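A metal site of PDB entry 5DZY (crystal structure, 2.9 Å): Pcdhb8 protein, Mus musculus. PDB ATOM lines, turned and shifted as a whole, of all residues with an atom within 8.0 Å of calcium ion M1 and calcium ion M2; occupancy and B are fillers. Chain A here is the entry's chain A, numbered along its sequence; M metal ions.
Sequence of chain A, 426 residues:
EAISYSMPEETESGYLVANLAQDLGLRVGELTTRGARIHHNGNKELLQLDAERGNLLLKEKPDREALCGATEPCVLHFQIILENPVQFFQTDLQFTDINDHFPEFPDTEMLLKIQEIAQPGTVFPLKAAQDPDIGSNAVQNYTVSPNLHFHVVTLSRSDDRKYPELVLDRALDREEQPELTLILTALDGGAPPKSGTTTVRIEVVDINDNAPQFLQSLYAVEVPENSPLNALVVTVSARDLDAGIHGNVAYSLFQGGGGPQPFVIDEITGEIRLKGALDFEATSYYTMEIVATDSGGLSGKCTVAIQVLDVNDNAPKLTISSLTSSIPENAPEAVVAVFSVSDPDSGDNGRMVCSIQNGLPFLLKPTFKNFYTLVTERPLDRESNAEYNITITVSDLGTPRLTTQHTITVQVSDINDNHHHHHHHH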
ATOM      1  N   GLU A 116     -12.086 -25.527  -1.311  1.00  0.00           N
ATOM      2  CA  GLU A 116     -11.957 -26.758  -2.089  1.00  0.00           C
ATOM      3  C   GLU A 116     -11.868 -28.006  -1.214  1.00  0.00           C
ATOM      4  O   GLU A 116     -12.396 -29.059  -1.573  1.00  0.00           O
ATOM      5  CB  GLU A 116     -10.736 -26.674  -2.999  1.00  0.00           C
ATOM      6  CG  GLU A 116     -10.489 -27.887  -3.882  1.00  0.00           C
ATOM      7  CD  GLU A 116      -9.212 -27.760  -4.690  1.00  0.00           C
ATOM      8  OE1 GLU A 116      -8.500 -26.743  -4.520  1.00  0.00           O
ATOM      9  OE2 GLU A 116      -8.906 -28.668  -5.486  1.00  0.00           O
ATOM     10  N   ILE A 117     -11.207 -27.896  -0.069  1.00  0.00           N
ATOM     11  CA  ILE A 117     -10.989 -29.055   0.804  1.00  0.00           C
ATOM     12  C   ILE A 117     -12.139 -29.295   1.783  1.00  0.00           C
ATOM     13  O   ILE A 117     -11.954 -29.964   2.799  1.00  0.00           O
ATOM     14  CB  ILE A 117      -9.690 -28.906   1.617  1.00  0.00           C
ATOM     15  CG1 ILE A 117      -9.687 -27.573   2.377  1.00  0.00           C
ATOM     16  CG2 ILE A 117      -8.475 -29.025   0.719  1.00  0.00           C
ATOM     17  CD1 ILE A 117      -8.441 -27.356   3.210  1.00  0.00           C
ATOM     18  N   LEU A 172     -15.413 -30.902  -3.606  1.00  0.00           N
ATOM     19  CA  LEU A 172     -15.254 -30.001  -4.747  1.00  0.00           C
ATOM     20  C   LEU A 172     -13.831 -30.007  -5.277  1.00  0.00           C
ATOM     21  O   LEU A 172     -12.925 -30.593  -4.683  1.00  0.00           O
ATOM     22  CB  LEU A 172     -15.659 -28.577  -4.359  1.00  0.00           C
ATOM     23  CG  LEU A 172     -17.097 -28.370  -3.862  1.00  0.00           C
ATOM     24  CD1 LEU A 172     -17.301 -26.934  -3.432  1.00  0.00           C
ATOM     25  CD2 LEU A 172     -18.086 -28.758  -4.943  1.00  0.00           C
ATOM     26  N   ASP A 173     -13.630 -29.323  -6.408  1.00  0.00           N
ATOM     27  CA  ASP A 173     -12.308 -29.202  -7.012  1.00  0.00           C
ATOM     28  C   ASP A 173     -12.288 -28.037  -8.000  1.00  0.00           C
ATOM     29  O   ASP A 173     -12.950 -28.089  -9.042  1.00  0.00           O
ATOM     30  CB  ASP A 173     -11.916 -30.504  -7.725  1.00  0.00           C
ATOM     31  CG  ASP A 173     -10.467 -30.492  -8.193  1.00  0.00           C
ATOM     32  OD1 ASP A 173      -9.588 -30.902  -7.403  1.00  0.00           O
ATOM     33  OD2 ASP A 173     -10.219 -30.081  -9.346  1.00  0.00           O
ATOM     34  N   ARG A 174     -11.544 -26.989  -7.663  1.00  0.00           N
ATOM     35  CA  ARG A 174     -11.481 -25.796  -8.499  1.00  0.00           C
ATOM     36  C   ARG A 174     -10.770 -26.081  -9.821  1.00  0.00           C
ATOM     37  O   ARG A 174     -11.034 -25.433 -10.833  1.00  0.00           O
ATOM     38  CB  ARG A 174     -10.765 -24.660  -7.762  1.00  0.00           C
ATOM     39  CG  ARG A 174     -10.864 -23.317  -8.465  1.00  0.00           C
ATOM     40  CD  ARG A 174      -9.850 -22.324  -7.930  1.00  0.00           C
ATOM     41  NE  ARG A 174      -8.489 -22.786  -8.154  1.00  0.00           N
ATOM     42  CZ  ARG A 174      -7.798 -22.572  -9.270  1.00  0.00           C
ATOM     43  NH1 ARG A 174      -6.555 -23.021  -9.378  1.00  0.00           N
ATOM     44  NH2 ARG A 174      -8.350 -21.915 -10.272  1.00  0.00           N
ATOM     45  N   GLU A 175      -9.864 -27.059  -9.800  1.00  0.00           N
ATOM     46  CA  GLU A 175      -9.111 -27.428 -10.985  1.00  0.00           C
ATOM     47  C   GLU A 175     -10.004 -28.141 -12.002  1.00  0.00           C
ATOM     48  O   GLU A 175      -9.672 -28.234 -13.179  1.00  0.00           O
ATOM     49  CB  GLU A 175      -7.919 -28.309 -10.620  1.00  0.00           C
ATOM     50  CG  GLU A 175      -6.785 -27.561  -9.919  1.00  0.00           C
ATOM     51  CD  GLU A 175      -7.145 -27.112  -8.513  1.00  0.00           C
ATOM     52  OE1 GLU A 175      -7.943 -27.806  -7.855  1.00  0.00           O
ATOM     53  OE2 GLU A 175      -6.645 -26.053  -8.075  1.00  0.00           O
ATOM     54  N   GLU A 176     -11.147 -28.646 -11.525  1.00  0.00           N
ATOM     55  CA  GLU A 176     -12.120 -29.289 -12.393  1.00  0.00           C
ATOM     56  C   GLU A 176     -13.273 -28.349 -12.714  1.00  0.00           C
ATOM     57  O   GLU A 176     -13.517 -28.019 -13.872  1.00  0.00           O
ATOM     58  CB  GLU A 176     -12.639 -30.571 -11.748  1.00  0.00           C
ATOM     59  N   VAL A 204     -16.065 -21.680  -5.614  1.00  0.00           N
ATOM     60  CA  VAL A 204     -15.065 -22.558  -5.022  1.00  0.00           C
ATOM     61  C   VAL A 204     -13.747 -21.826  -4.774  1.00  0.00           C
ATOM     62  O   VAL A 204     -13.038 -21.458  -5.715  1.00  0.00           O
ATOM     63  CB  VAL A 204     -14.793 -23.793  -5.905  1.00  0.00           C
ATOM     64  CG1 VAL A 204     -13.743 -24.683  -5.271  1.00  0.00           C
ATOM     65  CG2 VAL A 204     -16.081 -24.569  -6.130  1.00  0.00           C
ATOM     66  N   VAL A 205     -13.414 -21.635  -3.501  1.00  0.00           N
ATOM     67  CA  VAL A 205     -12.175 -20.968  -3.126  1.00  0.00           C
ATOM     68  C   VAL A 205     -10.976 -21.886  -3.361  1.00  0.00           C
ATOM     69  O   VAL A 205     -11.012 -23.059  -2.995  1.00  0.00           O
ATOM     70  CB  VAL A 205     -12.193 -20.531  -1.640  1.00  0.00           C
ATOM     71  CG1 VAL A 205     -10.892 -19.830  -1.277  1.00  0.00           C
ATOM     72  CG2 VAL A 205     -13.386 -19.628  -1.376  1.00  0.00           C
ATOM     73  N   ASP A 206      -9.930 -21.348  -3.977  1.00  0.00           N
ATOM     74  CA  ASP A 206      -8.740 -22.143  -4.297  1.00  0.00           C
ATOM     75  C   ASP A 206      -7.990 -22.603  -3.045  1.00  0.00           C
ATOM     76  O   ASP A 206      -7.745 -21.816  -2.136  1.00  0.00           O
ATOM     77  CB  ASP A 206      -7.791 -21.339  -5.187  1.00  0.00           C
ATOM     78  CG  ASP A 206      -6.542 -22.110  -5.553  1.00  0.00           C
ATOM     79  OD1 ASP A 206      -6.619 -23.349  -5.678  1.00  0.00           O
ATOM     80  OD2 ASP A 206      -5.470 -21.476  -5.723  1.00  0.00           O
ATOM     81  N   ILE A 207      -7.617 -23.881  -3.037  1.00  0.00           N
ATOM     82  CA  ILE A 207      -6.769 -24.418  -1.976  1.00  0.00           C
ATOM     83  C   ILE A 207      -5.530 -25.056  -2.590  1.00  0.00           C
ATOM     84  O   ILE A 207      -5.622 -25.775  -3.580  1.00  0.00           O
ATOM     85  CB  ILE A 207      -7.528 -25.463  -1.115  1.00  0.00           C
ATOM     86  CG1 ILE A 207      -8.784 -24.850  -0.498  1.00  0.00           C
ATOM     87  CG2 ILE A 207      -6.626 -25.998  -0.013  1.00  0.00           C
ATOM     88  CD1 ILE A 207      -8.501 -23.716   0.461  1.00  0.00           C
ATOM     89  N   ASN A 208      -4.362 -24.767  -2.006  1.00  0.00           N
ATOM     90  CA  ASN A 208      -3.103 -25.306  -2.506  1.00  0.00           C
ATOM     91  C   ASN A 208      -3.003 -26.797  -2.234  1.00  0.00           C
ATOM     92  O   ASN A 208      -2.404 -27.217  -1.234  1.00  0.00           O
ATOM     93  CB  ASN A 208      -1.919 -24.563  -1.892  1.00  0.00           C
ATOM     94  CG  ASN A 208      -0.571 -25.007  -2.465  1.00  0.00           C
ATOM     95  OD1 ASN A 208      -0.514 -25.711  -3.476  1.00  0.00           O
ATOM     96  ND2 ASN A 208       0.508 -24.593  -1.821  1.00  0.00           N
ATOM     97  N   ASP A 209      -3.605 -27.598  -3.101  1.00  0.00           N
ATOM     98  CA  ASP A 209      -3.571 -29.051  -2.970  1.00  0.00           C
ATOM     99  C   ASP A 209      -2.763 -29.667  -4.114  1.00  0.00           C
ATOM    100  O   ASP A 209      -2.645 -30.880  -4.227  1.00  0.00           O
ATOM    101  CB  ASP A 209      -4.992 -29.623  -2.932  1.00  0.00           C
ATOM    102  CG  ASP A 209      -5.812 -29.229  -4.149  1.00  0.00           C
ATOM    103  OD1 ASP A 209      -5.407 -28.304  -4.884  1.00  0.00           O
ATOM    104  OD2 ASP A 209      -6.880 -29.854  -4.370  1.00  0.00           O
ATOM    105  N   ASN A 210      -2.202 -28.801  -4.958  1.00  0.00           N
ATOM    106  CA  ASN A 210      -1.363 -29.240  -6.064  1.00  0.00           C
ATOM    107  C   ASN A 210       0.089 -28.795  -5.897  1.00  0.00           C
ATOM    108  O   ASN A 210       0.362 -27.649  -5.554  1.00  0.00           O
ATOM    109  CB  ASN A 210      -1.912 -28.725  -7.397  1.00  0.00           C
ATOM    110  CG  ASN A 210      -3.184 -29.430  -7.811  1.00  0.00           C
ATOM    111  OD1 ASN A 210      -3.133 -30.476  -8.463  1.00  0.00           O
ATOM    112  ND2 ASN A 210      -4.325 -28.866  -7.438  1.00  0.00           N
ATOM    113  N   ASP A 240       2.383 -24.606 -11.851  1.00  0.00           N
ATOM    114  CA  ASP A 240       1.488 -25.015 -10.773  1.00  0.00           C
ATOM    115  C   ASP A 240       0.048 -25.029 -11.262  1.00  0.00           C
ATOM    116  O   ASP A 240      -0.382 -24.146 -12.004  1.00  0.00           O
ATOM    117  CB  ASP A 240       1.640 -24.071  -9.578  1.00  0.00           C
ATOM    118  CG  ASP A 240       1.055 -24.650  -8.296  1.00  0.00           C
ATOM    119  OD1 ASP A 240       0.276 -25.620  -8.374  1.00  0.00           O
ATOM    120  OD2 ASP A 240       1.368 -24.113  -7.212  1.00  0.00           O
ATOM    121  N   LEU A 241      -0.711 -26.044 -10.842  1.00  0.00           N
ATOM    122  CA  LEU A 241      -2.093 -26.187 -11.255  1.00  0.00           C
ATOM    123  C   LEU A 241      -3.012 -25.240 -10.494  1.00  0.00           C
ATOM    124  O   LEU A 241      -4.104 -24.910 -10.960  1.00  0.00           O
ATOM    125  CB  LEU A 241      -2.563 -27.625 -11.078  1.00  0.00           C
ATOM    126  CG  LEU A 241      -1.851 -28.668 -11.953  1.00  0.00           C
ATOM    127  CD1 LEU A 241      -2.431 -30.057 -11.717  1.00  0.00           C
ATOM    128  CD2 LEU A 241      -1.941 -28.285 -13.417  1.00  0.00           C
ATOM    129  N   ASP A 242      -2.565 -24.788  -9.332  1.00  0.00           N
ATOM    130  CA  ASP A 242      -3.338 -23.843  -8.527  1.00  0.00           C
ATOM    131  C   ASP A 242      -3.194 -22.425  -9.074  1.00  0.00           C
ATOM    132  O   ASP A 242      -2.428 -22.183 -10.003  1.00  0.00           O
ATOM    133  CB  ASP A 242      -2.893 -23.892  -7.060  1.00  0.00           C
ATOM    134  CG  ASP A 242      -3.207 -25.224  -6.398  1.00  0.00           C
ATOM    135  OD1 ASP A 242      -4.216 -25.847  -6.791  1.00  0.00           O
ATOM    136  OD2 ASP A 242      -2.452 -25.635  -5.489  1.00  0.00           O
ATOM    137  N   ALA A 243      -3.933 -21.489  -8.482  1.00  0.00           N
ATOM    138  CA  ALA A 243      -3.901 -20.107  -8.923  1.00  0.00           C
ATOM    139  C   ALA A 243      -3.592 -19.152  -7.777  1.00  0.00           C
ATOM    140  O   ALA A 243      -3.693 -19.523  -6.611  1.00  0.00           O
ATOM    141  CB  ALA A 243      -5.232 -19.727  -9.574  1.00  0.00           C
ATOM    142  N   HIS A 246      -1.122 -19.345  -4.176  1.00  0.00           N
ATOM    143  CA  HIS A 246      -0.992 -20.795  -4.035  1.00  0.00           C
ATOM    144  C   HIS A 246      -0.354 -21.414  -5.272  1.00  0.00           C
ATOM    145  O   HIS A 246      -0.004 -22.589  -5.275  1.00  0.00           O
ATOM    146  CB  HIS A 246      -2.364 -21.426  -3.783  1.00  0.00           C
ATOM    147  CG  HIS A 246      -3.059 -20.895  -2.567  1.00  0.00           C
ATOM    148  ND1 HIS A 246      -3.120 -21.601  -1.384  1.00  0.00           N
ATOM    149  CD2 HIS A 246      -3.722 -19.741  -2.345  1.00  0.00           C
ATOM    150  CE1 HIS A 246      -3.794 -20.898  -0.483  1.00  0.00           C
ATOM    151  NE2 HIS A 246      -4.177 -19.759  -1.051  1.00  0.00           N
HETATM  152 CA    CA M   1      -7.471 -29.894  -6.571  1.00  0.00          CA
HETATM  153 CA    CA M   2      -6.469 -26.304  -5.814  1.00  0.00          CA
HETATM  154 CA    CA M   3       0.540 -25.103  -5.507  1.00  0.00          CA
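The backbone carbonyl oxygen (O) of Val 205 sits at hydrogen-bond distance from the backbone NH (N) of Glu 116, 3.2 Å away. The side-chain carboxylate (OD1) of Asp 209 lies close to the side-chain amide nitrogen (ND2) of Asn 210 (2.8 Å). The side-chain carboxylate (OD2) of Asp 173 lies within hydrogen-bond range of the backbone NH (N) of Glu 176, 2.8 Å away. N of Asn 210 is in hydrogen-bond range of OD2 of Asp 242 (3.2 Å). The side-chain carboxylate of Asp 242 sits close to the side-chain amide oxygen of Asn 208 (2.8 Å). OD1 of Asp 240 is in hydrogen-bond range of N of Asp 242 (3.1 Å). OD1 of Asp 206 lies within salt-bridge range of NE of Arg 174, 3.2 Å away. The backbone NH (N) of Ala 243 sits at hydrogen-bond distance from the side-chain carboxylate (OD2) of Asp 206, 3.2 Å away.
Asn 210 touches calcium ion M1 (ND2 to CA, 3.4 Å).
Residues that only touch calcium ion M2: Asn 210 (3.7 Å). Within 4 Å of calcium ion M2: Glu 116, Glu 175, Asp 206, Ile 207, Asp 209, Asn 210 and Asp 242.
Calcium ion M1 is bound by OE2 of Glu 116, 2.2 Å away. OD2 of Asp 209 is bound to calcium ion M1. OD1 of Asp 173 is bound to calcium ion M1 (2.5 Å). OE1 of Glu 175 binds calcium ion M1 (2.5 Å). Calcium ion M1 has four donor atoms within binding distance. Slightly farther from calcium ion M1 lies the side-chain carboxylate (OD1) of Asp 209 (3.1 Å).
Calcium ion M2 is bound by the side-chain carboxylate (OE2) of Glu 175 (2.3 Å), the backbone carbonyl oxygen (O) of Ile 207 (2.4 Å), the side-chain carboxylate (OD1) of Asp 209 (2.4 Å), the side-chain carboxylate (OE1) of Glu 116 (2.4 Å) and the side-chain carboxylate (OD1) of Asp 242 (2.5 Å). Slightly farther from calcium ion M2 lies the side-chain carboxylate (OE1) of Glu 175 (2.9 Å). Slightly farther from calcium ion M2 lies OD1 of Asp 206 (3.0 Å).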
